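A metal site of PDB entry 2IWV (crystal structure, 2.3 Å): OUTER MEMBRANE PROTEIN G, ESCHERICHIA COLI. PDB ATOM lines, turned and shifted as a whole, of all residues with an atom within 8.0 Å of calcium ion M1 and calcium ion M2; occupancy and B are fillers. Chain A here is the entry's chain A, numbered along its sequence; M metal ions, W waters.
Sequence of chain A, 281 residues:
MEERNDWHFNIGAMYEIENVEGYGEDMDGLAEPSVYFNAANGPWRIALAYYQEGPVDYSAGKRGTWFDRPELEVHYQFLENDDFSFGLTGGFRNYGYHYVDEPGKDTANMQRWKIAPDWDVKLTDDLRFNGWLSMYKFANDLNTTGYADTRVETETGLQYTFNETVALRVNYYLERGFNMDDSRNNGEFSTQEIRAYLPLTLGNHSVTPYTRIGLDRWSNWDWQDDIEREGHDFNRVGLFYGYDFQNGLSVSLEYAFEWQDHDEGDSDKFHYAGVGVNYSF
Calcium ion M2 is bound by water W2 (2.0 Å), water W1 (2.0 Å), the side-chain carboxylate of Glu 230 (2.3 Å) and the side-chain carboxylate of Asp 226 (2.4 Å).
Slightly farther from calcium ion M2 lies the side-chain carboxylate (OD1) of Asp 226 (3.0 Å).
The backbone carbonyl oxygen (O) of Ser 219 lies within hydrogen-bond range of the backbone NH (N) of Glu 230 (2.9 Å).
OD1 of Asn 220 lies close to O of Ile 227 (2.6 Å).
Calcium ion M1 is bound by OE2 of Glu 230 (1.8 Å), OD2 of Asp 222 (2.1 Å), OD2 of Asp 226 (2.1 Å), ND2 of Asn 220 (2.2 Å), O of Glu 228 (2.2 Å), O of Asp 226 (2.4 Å) and OE1 of Glu 230 (2.9 Å).
The nearest printed residue that does not touch calcium ion M1 is Arg 229 (4.4 Å).
Merely in contact with calcium ion M2: Glu 264.
The nearest printed residue that does not touch calcium ion M2 is Asp 222 (4.2 Å).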
ATOM      1  N   SER A 219       3.779  -7.309   7.291  1.00  0.00           N
ATOM      2  CA  SER A 219       2.849  -8.367   7.649  1.00  0.00           C
ATOM      3  C   SER A 219       3.624  -9.672   7.741  1.00  0.00           C
ATOM      4  O   SER A 219       4.797  -9.717   7.401  1.00  0.00           O
ATOM      5  CB  SER A 219       1.749  -8.451   6.583  1.00  0.00           C
ATOM      6  OG  SER A 219       2.281  -8.897   5.325  1.00  0.00           O
ATOM      7  N   ASN A 220       2.987 -10.714   8.241  1.00  0.00           N
ATOM      8  CA  ASN A 220       3.580 -12.060   8.184  1.00  0.00           C
ATOM      9  C   ASN A 220       2.484 -13.128   8.286  1.00  0.00           C
ATOM     10  O   ASN A 220       2.483 -13.991   9.186  1.00  0.00           O
ATOM     11  CB  ASN A 220       4.694 -12.226   9.237  1.00  0.00           C
ATOM     12  CG  ASN A 220       5.702 -13.304   8.891  1.00  0.00           C
ATOM     13  OD1 ASN A 220       6.493 -13.697   9.733  1.00  0.00           O
ATOM     14  ND2 ASN A 220       5.658 -13.817   7.681  1.00  0.00           N
ATOM     15  N   TRP A 221       1.554 -13.068   7.334  1.00  0.00           N
ATOM     16  CA  TRP A 221       0.441 -14.004   7.273  1.00  0.00           C
ATOM     17  C   TRP A 221       0.900 -15.399   6.869  1.00  0.00           C
ATOM     18  O   TRP A 221       0.212 -16.379   7.152  1.00  0.00           O
ATOM     19  CB  TRP A 221      -0.650 -13.520   6.337  1.00  0.00           C
ATOM     20  CG  TRP A 221      -0.921 -12.058   6.341  1.00  0.00           C
ATOM     21  CD1 TRP A 221      -0.623 -11.180   5.342  1.00  0.00           C
ATOM     22  CD2 TRP A 221      -1.573 -11.314   7.364  1.00  0.00           C
ATOM     23  NE1 TRP A 221      -1.027  -9.915   5.696  1.00  0.00           N
ATOM     24  CE2 TRP A 221      -1.609  -9.969   6.931  1.00  0.00           C
ATOM     25  CE3 TRP A 221      -2.110 -11.636   8.604  1.00  0.00           C
ATOM     26  CZ2 TRP A 221      -2.163  -8.940   7.708  1.00  0.00           C
ATOM     27  CZ3 TRP A 221      -2.672 -10.608   9.386  1.00  0.00           C
ATOM     28  CH2 TRP A 221      -2.696  -9.279   8.925  1.00  0.00           C
ATOM     29  N   ASP A 222       2.052 -15.482   6.219  1.00  0.00           N
ATOM     30  CA  ASP A 222       2.605 -16.763   5.797  1.00  0.00           C
ATOM     31  C   ASP A 222       3.707 -17.284   6.716  1.00  0.00           C
ATOM     32  O   ASP A 222       4.521 -18.141   6.341  1.00  0.00           O
ATOM     33  CB  ASP A 222       3.097 -16.682   4.341  1.00  0.00           C
ATOM     34  CG  ASP A 222       4.317 -15.796   4.178  1.00  0.00           C
ATOM     35  OD1 ASP A 222       4.707 -15.561   3.023  1.00  0.00           O
ATOM     36  OD2 ASP A 222       4.906 -15.337   5.175  1.00  0.00           O
ATOM     37  N   TRP A 223       3.749 -16.773   7.948  1.00  0.00           N
ATOM     38  CA  TRP A 223       4.855 -17.070   8.859  1.00  0.00           C
ATOM     39  C   TRP A 223       5.252 -18.547   8.985  1.00  0.00           C
ATOM     40  O   TRP A 223       6.429 -18.862   9.228  1.00  0.00           O
ATOM     41  CB  TRP A 223       4.571 -16.490  10.228  1.00  0.00           C
ATOM     42  CG  TRP A 223       3.475 -17.211  10.909  1.00  0.00           C
ATOM     43  CD1 TRP A 223       2.135 -16.921  10.837  1.00  0.00           C
ATOM     44  CD2 TRP A 223       3.605 -18.373  11.721  1.00  0.00           C
ATOM     45  NE1 TRP A 223       1.419 -17.822  11.585  1.00  0.00           N
ATOM     46  CE2 TRP A 223       2.303 -18.736  12.142  1.00  0.00           C
ATOM     47  CE3 TRP A 223       4.689 -19.141  12.160  1.00  0.00           C
ATOM     48  CZ2 TRP A 223       2.064 -19.845  12.966  1.00  0.00           C
ATOM     49  CZ3 TRP A 223       4.458 -20.268  12.969  1.00  0.00           C
ATOM     50  CH2 TRP A 223       3.161 -20.597  13.366  1.00  0.00           C
ATOM     51  N   GLN A 224       4.276 -19.457   8.819  1.00  0.00           N
ATOM     52  CA  GLN A 224       4.486 -20.898   9.084  1.00  0.00           C
ATOM     53  C   GLN A 224       5.345 -21.553   8.036  1.00  0.00           C
ATOM     54  O   GLN A 224       6.055 -22.528   8.330  1.00  0.00           O
ATOM     55  CB  GLN A 224       3.163 -21.673   9.208  1.00  0.00           C
ATOM     56  CG  GLN A 224       3.329 -23.155   9.535  1.00  0.00           C
ATOM     57  CD  GLN A 224       3.702 -23.440  10.994  1.00  0.00           C
ATOM     58  OE1 GLN A 224       2.823 -23.781  11.828  1.00  0.00           O
ATOM     59  NE2 GLN A 224       5.001 -23.311  11.325  1.00  0.00           N
ATOM     60  N   ASP A 225       5.296 -21.035   6.822  1.00  0.00           N
ATOM     61  CA  ASP A 225       6.175 -21.514   5.759  1.00  0.00           C
ATOM     62  C   ASP A 225       7.305 -20.526   5.453  1.00  0.00           C
ATOM     63  O   ASP A 225       8.390 -20.947   5.001  1.00  0.00           O
ATOM     64  CB  ASP A 225       5.376 -21.835   4.487  1.00  0.00           C
ATOM     65  CG  ASP A 225       4.324 -22.908   4.712  1.00  0.00           C
ATOM     66  OD1 ASP A 225       4.694 -24.108   4.879  1.00  0.00           O
ATOM     67  OD2 ASP A 225       3.124 -22.559   4.754  1.00  0.00           O
ATOM     68  N   ASP A 226       7.052 -19.233   5.708  1.00  0.00           N
ATOM     69  CA  ASP A 226       8.028 -18.159   5.462  1.00  0.00           C
ATOM     70  C   ASP A 226       8.088 -17.184   6.631  1.00  0.00           C
ATOM     71  O   ASP A 226       7.365 -16.209   6.683  1.00  0.00           O
ATOM     72  CB  ASP A 226       7.643 -17.485   4.171  1.00  0.00           C
ATOM     73  CG  ASP A 226       8.373 -16.169   3.931  1.00  0.00           C
ATOM     74  OD1 ASP A 226       9.534 -16.216   3.465  1.00  0.00           O
ATOM     75  OD2 ASP A 226       7.749 -15.097   4.193  1.00  0.00           O
ATOM     76  N   ILE A 227       8.972 -17.452   7.577  1.00  0.00           N
ATOM     77  CA  ILE A 227       8.935 -16.819   8.924  1.00  0.00           C
ATOM     78  C   ILE A 227       9.319 -15.365   8.930  1.00  0.00           C
ATOM     79  O   ILE A 227       8.907 -14.651   9.834  1.00  0.00           O
ATOM     80  CB  ILE A 227       9.792 -17.604   9.968  1.00  0.00           C
ATOM     81  CG1 ILE A 227       9.455 -17.196  11.378  1.00  0.00           C
ATOM     82  CG2 ILE A 227      11.298 -17.434   9.736  1.00  0.00           C
ATOM     83  CD1 ILE A 227      10.331 -17.947  12.403  1.00  0.00           C
ATOM     84  N   GLU A 228      10.076 -14.914   7.934  1.00  0.00           N
ATOM     85  CA  GLU A 228      10.371 -13.490   7.804  1.00  0.00           C
ATOM     86  C   GLU A 228       9.203 -12.669   7.318  1.00  0.00           C
ATOM     87  O   GLU A 228       8.268 -13.182   6.693  1.00  0.00           O
ATOM     88  CB  GLU A 228      11.679 -13.240   7.028  1.00  0.00           C
ATOM     89  CG  GLU A 228      12.952 -13.448   7.976  1.00  0.00           C
ATOM     90  CD  GLU A 228      14.223 -12.658   7.591  1.00  0.00           C
ATOM     91  OE1 GLU A 228      15.330 -13.254   7.574  1.00  0.00           O
ATOM     92  OE2 GLU A 228      14.124 -11.425   7.326  1.00  0.00           O
ATOM     93  N   ARG A 229       9.259 -11.382   7.620  1.00  0.00           N
ATOM     94  CA  ARG A 229       8.131 -10.441   7.469  1.00  0.00           C
ATOM     95  C   ARG A 229       8.173  -9.898   6.093  1.00  0.00           C
ATOM     96  O   ARG A 229       9.268  -9.745   5.552  1.00  0.00           O
ATOM     97  CB  ARG A 229       8.266  -9.313   8.488  1.00  0.00           C
ATOM     98  CG  ARG A 229       7.566  -9.650   9.779  1.00  0.00           C
ATOM     99  CD  ARG A 229       8.412  -9.596  11.057  1.00  0.00           C
ATOM    100  NE  ARG A 229       9.070  -8.323  11.364  1.00  0.00           N
ATOM    101  CZ  ARG A 229       9.195  -7.863  12.612  1.00  0.00           C
ATOM    102  NH1 ARG A 229       8.684  -8.541  13.679  1.00  0.00           N
ATOM    103  NH2 ARG A 229       9.823  -6.707  12.809  1.00  0.00           N
ATOM    104  N   GLU A 230       6.988  -9.638   5.512  1.00  0.00           N
ATOM    105  CA  GLU A 230       6.874  -9.018   4.187  1.00  0.00           C
ATOM    106  C   GLU A 230       6.614  -7.539   4.372  1.00  0.00           C
ATOM    107  O   GLU A 230       5.779  -7.165   5.172  1.00  0.00           O
ATOM    108  CB  GLU A 230       5.733  -9.612   3.368  1.00  0.00           C
ATOM    109  CG  GLU A 230       5.079 -10.926   3.826  1.00  0.00           C
ATOM    110  CD  GLU A 230       6.013 -12.040   4.300  1.00  0.00           C
ATOM    111  OE1 GLU A 230       7.078 -12.269   3.698  1.00  0.00           O
ATOM    112  OE2 GLU A 230       5.650 -12.741   5.268  1.00  0.00           O
ATOM    113  N   GLY A 231       7.359  -6.697   3.643  1.00  0.00           N
ATOM    114  CA  GLY A 231       7.216  -5.246   3.732  1.00  0.00           C
ATOM    115  C   GLY A 231       6.332  -4.693   2.640  1.00  0.00           C
ATOM    116  O   GLY A 231       6.128  -5.386   1.651  1.00  0.00           O
ATOM    117  N   GLU A 264       7.802  -7.988  -2.143  1.00  0.00           N
ATOM    118  CA  GLU A 264       7.653  -9.152  -2.982  1.00  0.00           C
ATOM    119  C   GLU A 264       6.213  -9.383  -3.395  1.00  0.00           C
ATOM    120  O   GLU A 264       5.342  -9.672  -2.574  1.00  0.00           O
ATOM    121  CB  GLU A 264       8.193 -10.404  -2.301  1.00  0.00           C
ATOM    122  CG  GLU A 264       7.831 -10.538  -0.849  1.00  0.00           C
ATOM    123  CD  GLU A 264       9.040 -10.509   0.068  1.00  0.00           C
ATOM    124  OE1 GLU A 264       9.263  -9.473   0.728  1.00  0.00           O
ATOM    125  OE2 GLU A 264       9.772 -11.523   0.121  1.00  0.00           O
HETATM  126 CA    CA M   1       6.542 -14.221   5.709  1.00  0.00          CA
HETATM  127 CA    CA M   2       8.428 -13.648   2.369  1.00  0.00          CA
HETATM  128  O   HOH W   1       9.324 -11.814   2.495  1.00  0.00           O
HETATM  129  O   HOH W   2       7.018 -14.673   1.331  1.00  0.00           O
